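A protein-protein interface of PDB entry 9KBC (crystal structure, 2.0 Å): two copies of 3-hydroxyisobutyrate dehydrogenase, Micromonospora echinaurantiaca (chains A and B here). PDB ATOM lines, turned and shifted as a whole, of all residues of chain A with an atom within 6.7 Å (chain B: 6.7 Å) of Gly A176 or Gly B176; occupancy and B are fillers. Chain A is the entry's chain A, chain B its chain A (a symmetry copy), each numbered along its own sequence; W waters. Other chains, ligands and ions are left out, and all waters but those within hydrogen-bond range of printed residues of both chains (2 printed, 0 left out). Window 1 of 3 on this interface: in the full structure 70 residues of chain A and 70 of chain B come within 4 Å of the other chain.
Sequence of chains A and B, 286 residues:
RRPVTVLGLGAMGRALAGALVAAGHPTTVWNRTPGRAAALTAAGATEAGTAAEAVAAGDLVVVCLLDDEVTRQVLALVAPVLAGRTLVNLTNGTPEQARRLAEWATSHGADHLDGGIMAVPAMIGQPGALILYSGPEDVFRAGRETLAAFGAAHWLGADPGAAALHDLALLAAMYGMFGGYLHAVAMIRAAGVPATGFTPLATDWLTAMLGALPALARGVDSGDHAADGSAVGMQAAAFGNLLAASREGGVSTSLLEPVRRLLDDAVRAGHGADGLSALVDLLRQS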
ATOM      1  N   LEU A 171      -5.365  15.667  -7.935  1.00  0.00           N
ATOM      2  CA  LEU A 171      -4.466  14.885  -8.780  1.00  0.00           C
ATOM      3  C   LEU A 171      -5.218  14.245  -9.941  1.00  0.00           C
ATOM      4  O   LEU A 171      -4.720  14.219 -11.073  1.00  0.00           O
ATOM      5  CB  LEU A 171      -3.759  13.816  -7.949  1.00  0.00           C
ATOM      6  CG  LEU A 171      -2.650  14.318  -7.021  1.00  0.00           C
ATOM      7  CD1 LEU A 171      -1.878  13.152  -6.419  1.00  0.00           C
ATOM      8  CD2 LEU A 171      -1.722  15.261  -7.765  1.00  0.00           C
ATOM      9  N   ALA A 172      -6.415  13.716  -9.676  1.00  0.00           N
ATOM     10  CA  ALA A 172      -7.223  13.131 -10.742  1.00  0.00           C
ATOM     11  C   ALA A 172      -7.544  14.161 -11.816  1.00  0.00           C
ATOM     12  O   ALA A 172      -7.436  13.875 -13.014  1.00  0.00           O
ATOM     13  CB  ALA A 172      -8.513  12.545 -10.164  1.00  0.00           C
ATOM     14  N   ALA A 173      -7.939  15.366 -11.402  1.00  0.00           N
ATOM     15  CA  ALA A 173      -8.231  16.425 -12.361  1.00  0.00           C
ATOM     16  C   ALA A 173      -6.996  16.786 -13.178  1.00  0.00           C
ATOM     17  O   ALA A 173      -7.089  17.022 -14.390  1.00  0.00           O
ATOM     18  CB  ALA A 173      -8.772  17.655 -11.628  1.00  0.00           C
ATOM     19  N   MET A 174      -5.830  16.825 -12.532  1.00  0.00           N
ATOM     20  CA  MET A 174      -4.592  17.164 -13.229  1.00  0.00           C
ATOM     21  C   MET A 174      -4.206  16.086 -14.236  1.00  0.00           C
ATOM     22  O   MET A 174      -3.824  16.397 -15.370  1.00  0.00           O
ATOM     23  CB  MET A 174      -3.473  17.390 -12.209  1.00  0.00           C
ATOM     24  CG  MET A 174      -2.068  17.439 -12.792  1.00  0.00           C
ATOM     25  SD  MET A 174      -0.779  17.194 -11.540  1.00  0.00           S
ATOM     26  CE  MET A 174      -0.533  15.425 -11.628  1.00  0.00           C
ATOM     27  N   TYR A 175      -4.306  14.816 -13.843  1.00  0.00           N
ATOM     28  CA  TYR A 175      -3.964  13.724 -14.751  1.00  0.00           C
ATOM     29  C   TYR A 175      -4.888  13.696 -15.960  1.00  0.00           C
ATOM     30  O   TYR A 175      -4.455  13.380 -17.076  1.00  0.00           O
ATOM     31  CB  TYR A 175      -4.013  12.404 -13.990  1.00  0.00           C
ATOM     32  CG  TYR A 175      -2.753  12.145 -13.204  1.00  0.00           C
ATOM     33  CD1 TYR A 175      -1.510  12.457 -13.736  1.00  0.00           C
ATOM     34  CD2 TYR A 175      -2.809  11.664 -11.906  1.00  0.00           C
ATOM     35  CE1 TYR A 175      -0.353  12.238 -13.021  1.00  0.00           C
ATOM     36  CE2 TYR A 175      -1.656  11.449 -11.175  1.00  0.00           C
ATOM     37  CZ  TYR A 175      -0.431  11.740 -11.739  1.00  0.00           C
ATOM     38  OH  TYR A 175       0.723  11.532 -11.019  1.00  0.00           O
ATOM     39  N   GLY A 176      -6.164  14.031 -15.761  1.00  0.00           N
ATOM     40  CA  GLY A 176      -7.077  14.121 -16.888  1.00  0.00           C
ATOM     41  C   GLY A 176      -6.691  15.214 -17.867  1.00  0.00           C
ATOM     42  O   GLY A 176      -6.596  14.975 -19.074  1.00  0.00           O
ATOM     43  N   MET A 177      -6.483  16.437 -17.358  1.00  0.00           N
ATOM     44  CA  MET A 177      -5.979  17.529 -18.191  1.00  0.00           C
ATOM     45  C   MET A 177      -4.729  17.129 -18.957  1.00  0.00           C
ATOM     46  O   MET A 177      -4.658  17.287 -20.180  1.00  0.00           O
ATOM     47  CB  MET A 177      -5.655  18.769 -17.355  1.00  0.00           C
ATOM     48  CG  MET A 177      -5.526  20.015 -18.232  1.00  0.00           C
ATOM     49  SD  MET A 177      -5.976  21.578 -17.477  1.00  0.00           S
ATOM     50  CE  MET A 177      -4.825  21.614 -16.117  1.00  0.00           C
ATOM     51  N   PHE A 178      -3.713  16.646 -18.241  1.00  0.00           N
ATOM     52  CA  PHE A 178      -2.441  16.357 -18.890  1.00  0.00           C
ATOM     53  C   PHE A 178      -2.594  15.245 -19.914  1.00  0.00           C
ATOM     54  O   PHE A 178      -2.069  15.345 -21.029  1.00  0.00           O
ATOM     55  CB  PHE A 178      -1.388  15.995 -17.844  1.00  0.00           C
ATOM     56  CG  PHE A 178      -0.833  17.183 -17.109  1.00  0.00           C
ATOM     57  CD1 PHE A 178      -0.956  18.461 -17.636  1.00  0.00           C
ATOM     58  CD2 PHE A 178      -0.194  17.026 -15.890  1.00  0.00           C
ATOM     59  CE1 PHE A 178      -0.447  19.558 -16.960  1.00  0.00           C
ATOM     60  CE2 PHE A 178       0.320  18.119 -15.214  1.00  0.00           C
ATOM     61  CZ  PHE A 178       0.190  19.385 -15.749  1.00  0.00           C
ATOM     62  N   GLY A 179      -3.328  14.187 -19.564  1.00  0.00           N
ATOM     63  CA  GLY A 179      -3.565  13.117 -20.517  1.00  0.00           C
ATOM     64  C   GLY A 179      -4.222  13.613 -21.792  1.00  0.00           C
ATOM     65  O   GLY A 179      -3.822  13.233 -22.894  1.00  0.00           O
ATOM     66  N   GLY A 180      -5.231  14.477 -21.657  1.00  0.00           N
ATOM     67  CA  GLY A 180      -5.877  15.036 -22.832  1.00  0.00           C
ATOM     68  C   GLY A 180      -4.966  15.962 -23.615  1.00  0.00           C
ATOM     69  O   GLY A 180      -4.974  15.956 -24.848  1.00  0.00           O
ATOM     70  N   TYR A 181      -4.173  16.774 -22.911  1.00  0.00           N
ATOM     71  CA  TYR A 181      -3.210  17.630 -23.593  1.00  0.00           C
ATOM     72  C   TYR A 181      -2.148  16.801 -24.304  1.00  0.00           C
ATOM     73  O   TYR A 181      -1.789  17.093 -25.452  1.00  0.00           O
ATOM     74  CB  TYR A 181      -2.562  18.594 -22.598  1.00  0.00           C
ATOM     75  CG  TYR A 181      -1.394  19.370 -23.170  1.00  0.00           C
ATOM     76  CD1 TYR A 181      -1.599  20.525 -23.916  1.00  0.00           C
ATOM     77  CD2 TYR A 181      -0.088  18.945 -22.966  1.00  0.00           C
ATOM     78  CE1 TYR A 181      -0.532  21.238 -24.439  1.00  0.00           C
ATOM     79  CE2 TYR A 181       0.981  19.646 -23.487  1.00  0.00           C
ATOM     80  CZ  TYR A 181       0.756  20.792 -24.220  1.00  0.00           C
ATOM     81  OH  TYR A 181       1.824  21.490 -24.738  1.00  0.00           O
ATOM     82  N   LEU A 255      -6.128   6.775 -24.155  1.00  0.00           N
ATOM     83  CA  LEU A 255      -6.469   7.788 -23.162  1.00  0.00           C
ATOM     84  C   LEU A 255      -7.918   8.242 -23.285  1.00  0.00           C
ATOM     85  O   LEU A 255      -8.514   8.685 -22.296  1.00  0.00           O
ATOM     86  CB  LEU A 255      -5.533   8.988 -23.288  1.00  0.00           C
ATOM     87  CG  LEU A 255      -4.057   8.704 -23.020  1.00  0.00           C
ATOM     88  CD1 LEU A 255      -3.233   9.976 -23.152  1.00  0.00           C
ATOM     89  CD2 LEU A 255      -3.878   8.079 -21.642  1.00  0.00           C
ATOM     90  N   LEU A 256      -8.499   8.135 -24.480  1.00  0.00           N
ATOM     91  CA  LEU A 256      -9.830   8.666 -24.748  1.00  0.00           C
ATOM     92  C   LEU A 256     -10.932   7.618 -24.719  1.00  0.00           C
ATOM     93  O   LEU A 256     -12.098   7.985 -24.526  1.00  0.00           O
ATOM     94  CB  LEU A 256      -9.859   9.357 -26.115  1.00  0.00           C
ATOM     95  CG  LEU A 256      -8.786  10.404 -26.405  1.00  0.00           C
ATOM     96  CD1 LEU A 256      -8.849  10.798 -27.874  1.00  0.00           C
ATOM     97  CD2 LEU A 256      -8.957  11.618 -25.516  1.00  0.00           C
ATOM     98  N   VAL A 259     -13.503   7.737 -21.826  1.00  0.00           N
ATOM     99  CA  VAL A 259     -14.449   8.845 -21.914  1.00  0.00           C
ATOM    100  C   VAL A 259     -15.491   8.561 -22.987  1.00  0.00           C
ATOM    101  O   VAL A 259     -16.673   8.892 -22.829  1.00  0.00           O
ATOM    102  CB  VAL A 259     -13.709  10.171 -22.175  1.00  0.00           C
ATOM    103  CG1 VAL A 259     -14.685  11.336 -22.113  1.00  0.00           C
ATOM    104  CG2 VAL A 259     -12.594  10.364 -21.163  1.00  0.00           C
ATOM    105  N   LEU B 171     -10.527  19.173 -28.768  1.00  0.00           N
ATOM    106  CA  LEU B 171     -11.551  18.324 -28.167  1.00  0.00           C
ATOM    107  C   LEU B 171     -10.930  17.269 -27.259  1.00  0.00           C
ATOM    108  O   LEU B 171     -11.451  16.991 -26.172  1.00  0.00           O
ATOM    109  CB  LEU B 171     -12.392  17.661 -29.256  1.00  0.00           C
ATOM    110  CG  LEU B 171     -13.392  18.571 -29.974  1.00  0.00           C
ATOM    111  CD1 LEU B 171     -14.316  17.759 -30.871  1.00  0.00           C
ATOM    112  CD2 LEU B 171     -14.185  19.385 -28.968  1.00  0.00           C
ATOM    113  N   ALA B 172      -9.820  16.666 -27.693  1.00  0.00           N
ATOM    114  CA  ALA B 172      -9.133  15.683 -26.861  1.00  0.00           C
ATOM    115  C   ALA B 172      -8.686  16.297 -25.542  1.00  0.00           C
ATOM    116  O   ALA B 172      -8.862  15.695 -24.476  1.00  0.00           O
ATOM    117  CB  ALA B 172      -7.933  15.104 -27.613  1.00  0.00           C
ATOM    118  N   ALA B 173      -8.105  17.497 -25.596  1.00  0.00           N
ATOM    119  CA  ALA B 173      -7.679  18.176 -24.378  1.00  0.00           C
ATOM    120  C   ALA B 173      -8.864  18.464 -23.464  1.00  0.00           C
ATOM    121  O   ALA B 173      -8.764  18.322 -22.238  1.00  0.00           O
ATOM    122  CB  ALA B 173      -6.944  19.469 -24.735  1.00  0.00           C
ATOM    123  N   MET B 174      -9.997  18.863 -24.045  1.00  0.00           N
ATOM    124  CA  MET B 174     -11.184  19.167 -23.252  1.00  0.00           C
ATOM    125  C   MET B 174     -11.751  17.914 -22.593  1.00  0.00           C
ATOM    126  O   MET B 174     -12.107  17.936 -21.410  1.00  0.00           O
ATOM    127  CB  MET B 174     -12.234  19.845 -24.137  1.00  0.00           C
ATOM    128  CG  MET B 174     -13.629  19.933 -23.534  1.00  0.00           C
ATOM    129  SD  MET B 174     -14.911  20.258 -24.774  1.00  0.00           S
ATOM    130  CE  MET B 174     -15.422  18.597 -25.197  1.00  0.00           C
ATOM    131  N   TYR B 175     -11.834  16.813 -23.340  1.00  0.00           N
ATOM    132  CA  TYR B 175     -12.356  15.569 -22.781  1.00  0.00           C
ATOM    133  C   TYR B 175     -11.473  15.053 -21.652  1.00  0.00           C
ATOM    134  O   TYR B 175     -11.974  14.495 -20.667  1.00  0.00           O
ATOM    135  CB  TYR B 175     -12.488  14.535 -23.892  1.00  0.00           C
ATOM    136  CG  TYR B 175     -13.755  14.707 -24.691  1.00  0.00           C
ATOM    137  CD1 TYR B 175     -14.948  15.034 -24.064  1.00  0.00           C
ATOM    138  CD2 TYR B 175     -13.742  14.621 -26.074  1.00  0.00           C
ATOM    139  CE1 TYR B 175     -16.109  15.208 -24.786  1.00  0.00           C
ATOM    140  CE2 TYR B 175     -14.898  14.803 -26.809  1.00  0.00           C
ATOM    141  CZ  TYR B 175     -16.078  15.098 -26.159  1.00  0.00           C
ATOM    142  OH  TYR B 175     -17.233  15.282 -26.882  1.00  0.00           O
ATOM    143  N   GLY B 176     -10.158  15.236 -21.773  1.00  0.00           N
ATOM    144  CA  GLY B 176      -9.266  14.857 -20.690  1.00  0.00           C
ATOM    145  C   GLY B 176      -9.506  15.664 -19.428  1.00  0.00           C
ATOM    146  O   GLY B 176      -9.663  15.102 -18.340  1.00  0.00           O
ATOM    147  N   MET B 177      -9.517  16.999 -19.555  1.00  0.00           N
ATOM    148  CA  MET B 177      -9.870  17.865 -18.430  1.00  0.00           C
ATOM    149  C   MET B 177     -11.183  17.452 -17.785  1.00  0.00           C
ATOM    150  O   MET B 177     -11.256  17.257 -16.567  1.00  0.00           O
ATOM    151  CB  MET B 177      -9.986  19.327 -18.862  1.00  0.00           C
ATOM    152  CG  MET B 177      -9.946  20.270 -17.659  1.00  0.00           C
ATOM    153  SD  MET B 177      -9.250  21.899 -17.937  1.00  0.00           S
ATOM    154  CE  MET B 177     -10.352  22.500 -19.203  1.00  0.00           C
ATOM    155  N   PHE B 178     -12.243  17.355 -18.588  1.00  0.00           N
ATOM    156  CA  PHE B 178     -13.559  17.084 -18.023  1.00  0.00           C
ATOM    157  C   PHE B 178     -13.597  15.713 -17.368  1.00  0.00           C
ATOM    158  O   PHE B 178     -14.126  15.563 -16.261  1.00  0.00           O
ATOM    159  CB  PHE B 178     -14.631  17.204 -19.104  1.00  0.00           C
ATOM    160  CG  PHE B 178     -14.985  18.623 -19.450  1.00  0.00           C
ATOM    161  CD1 PHE B 178     -14.683  19.659 -18.579  1.00  0.00           C
ATOM    162  CD2 PHE B 178     -15.612  18.924 -20.648  1.00  0.00           C
ATOM    163  CE1 PHE B 178     -15.006  20.969 -18.896  1.00  0.00           C
ATOM    164  CE2 PHE B 178     -15.941  20.230 -20.966  1.00  0.00           C
ATOM    165  CZ  PHE B 178     -15.635  21.252 -20.089  1.00  0.00           C
ATOM    166  N   GLY B 179     -13.022  14.705 -18.027  1.00  0.00           N
ATOM    167  CA  GLY B 179     -12.970  13.382 -17.431  1.00  0.00           C
ATOM    168  C   GLY B 179     -12.274  13.381 -16.082  1.00  0.00           C
ATOM    169  O   GLY B 179     -12.752  12.763 -15.129  1.00  0.00           O
ATOM    170  N   GLY B 180     -11.145  14.086 -15.983  1.00  0.00           N
ATOM    171  CA  GLY B 180     -10.448  14.177 -14.711  1.00  0.00           C
ATOM    172  C   GLY B 180     -11.227  14.961 -13.673  1.00  0.00           C
ATOM    173  O   GLY B 180     -11.249  14.596 -12.495  1.00  0.00           O
ATOM    174  N   TYR B 181     -11.874  16.052 -14.093  1.00  0.00           N
ATOM    175  CA  TYR B 181     -12.713  16.807 -13.170  1.00  0.00           C
ATOM    176  C   TYR B 181     -13.903  15.977 -12.708  1.00  0.00           C
ATOM    177  O   TYR B 181     -14.239  15.974 -11.516  1.00  0.00           O
ATOM    178  CB  TYR B 181     -13.187  18.104 -13.828  1.00  0.00           C
ATOM    179  CG  TYR B 181     -14.238  18.847 -13.030  1.00  0.00           C
ATOM    180  CD1 TYR B 181     -13.879  19.691 -11.985  1.00  0.00           C
ATOM    181  CD2 TYR B 181     -15.588  18.700 -13.319  1.00  0.00           C
ATOM    182  CE1 TYR B 181     -14.838  20.373 -11.254  1.00  0.00           C
ATOM    183  CE2 TYR B 181     -16.551  19.372 -12.593  1.00  0.00           C
ATOM    184  CZ  TYR B 181     -16.173  20.209 -11.565  1.00  0.00           C
ATOM    185  OH  TYR B 181     -17.135  20.878 -10.842  1.00  0.00           O
ATOM    186  N   LEU B 255     -11.469   5.947 -15.848  1.00  0.00           N
ATOM    187  CA  LEU B 255     -10.958   7.142 -16.512  1.00  0.00           C
ATOM    188  C   LEU B 255      -9.460   7.318 -16.295  1.00  0.00           C
ATOM    189  O   LEU B 255      -8.782   7.934 -17.127  1.00  0.00           O
ATOM    190  CB  LEU B 255     -11.706   8.380 -16.022  1.00  0.00           C
ATOM    191  CG  LEU B 255     -13.201   8.410 -16.328  1.00  0.00           C
ATOM    192  CD1 LEU B 255     -13.828   9.698 -15.814  1.00  0.00           C
ATOM    193  CD2 LEU B 255     -13.441   8.246 -17.824  1.00  0.00           C
ATOM    194  N   LEU B 256      -8.928   6.783 -15.196  1.00  0.00           N
ATOM    195  CA  LEU B 256      -7.540   7.008 -14.815  1.00  0.00           C
ATOM    196  C   LEU B 256      -6.606   5.860 -15.172  1.00  0.00           C
ATOM    197  O   LEU B 256      -5.394   6.088 -15.276  1.00  0.00           O
ATOM    198  CB  LEU B 256      -7.438   7.260 -13.308  1.00  0.00           C
ATOM    199  CG  LEU B 256      -8.347   8.325 -12.702  1.00  0.00           C
ATOM    200  CD1 LEU B 256      -8.259   8.263 -11.184  1.00  0.00           C
ATOM    201  CD2 LEU B 256      -7.977   9.705 -13.205  1.00  0.00           C
ATOM    202  N   VAL B 259      -3.982   6.426 -17.962  1.00  0.00           N
ATOM    203  CA  VAL B 259      -2.884   7.307 -17.578  1.00  0.00           C
ATOM    204  C   VAL B 259      -1.920   6.571 -16.657  1.00  0.00           C
ATOM    205  O   VAL B 259      -0.699   6.752 -16.738  1.00  0.00           O
ATOM    206  CB  VAL B 259      -3.421   8.595 -16.927  1.00  0.00           C
ATOM    207  CG1 VAL B 259      -2.281   9.568 -16.670  1.00  0.00           C
ATOM    208  CG2 VAL B 259      -4.473   9.239 -17.814  1.00  0.00           C
HETATM  209  O   HOH W   1      -9.460  18.260 -15.049  1.00  0.00           O
HETATM  210  O   HOH W   2      -6.250  18.945 -21.302  1.00  0.00           O
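Of the 14 printed residues of chain A, 5 touch a printed residue of chain B.
Hydrophobic or aromatic side chains of chain A that line the printed part of chain B: Met A177.
Printed residues of chain B that touch a printed residue of chain A: Ala B172, Ala B173, Gly B176, Met B177 and Gly B180.
Hydrophobic or aromatic side chains of chain B within 4 Å of the printed part of chain A: Met B177.
Among the printed residues, 8 pairs touch across the chains.
Water W1 lies within hydrogen-bond range of O of Met B177, O of Ala A173 and N of Tyr B181.
Water W2 lies within hydrogen-bond range of the backbone carbonyl oxygen of Met A177, the backbone carbonyl oxygen of Ala B173 and the backbone NH of Tyr A181.
The backbone carbonyl oxygen (O) of Gly B176 sits close to the backbone carbonyl oxygen (O) of Gly A176, 3.2 Å away.
The side-chain sulfur of Met A177 lies close to the side-chain sulfur of Met B177 (3.3 Å).
Ala A172 touches Gly B180, and with the chains exchanged Gly A180 touches Ala B172.
Ala A173 touches Gly B180, and with the chains exchanged Gly A180 touches Ala B173.
Gly B176 touches its own counterpart, Gly A176.
Gly A176 touches Met B177, and with the chains exchanged Met A177 touches Gly B176.
Of the printed residues of chain B, Gly A176 touches Gly B176 (3.0 Å) and Met B177 (3.6 Å).
Of the printed residues of chain A, Gly B176 touches Gly A176 and Met A177.
Of the printed residues of chain B, Met A177 touches Gly B176 and Met B177.
Of the printed residues of chain B, Ala A173 touches Gly B180.
Printed residues of chain A within 4 Å of Ala B173: Gly A180.
Of the printed residues of chain B, Ala A172 touches Gly B180 (3.5 Å).
Tyr A175 touches none of the printed residues of chain B.
The nearest printed residue of chain A that does not touch Gly B176 is Gly A180 (4.01 Å).
The nearest printed residue of chain A that does not touch Met B177 is Ala A173 (4.7 Å).
Among the printed residues, merely in contact across the chains: Ala A172 with Gly B180 (3.5 Å), Ala A173 with Gly B180 (3.5 Å), Gly A176 with Met B177 (3.6 Å), Met A177 with Gly B176 (3.6 Å), Gly A180 with Ala B172 (3.5 Å) and Gly A180 with Ala B173 (3.5 Å).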
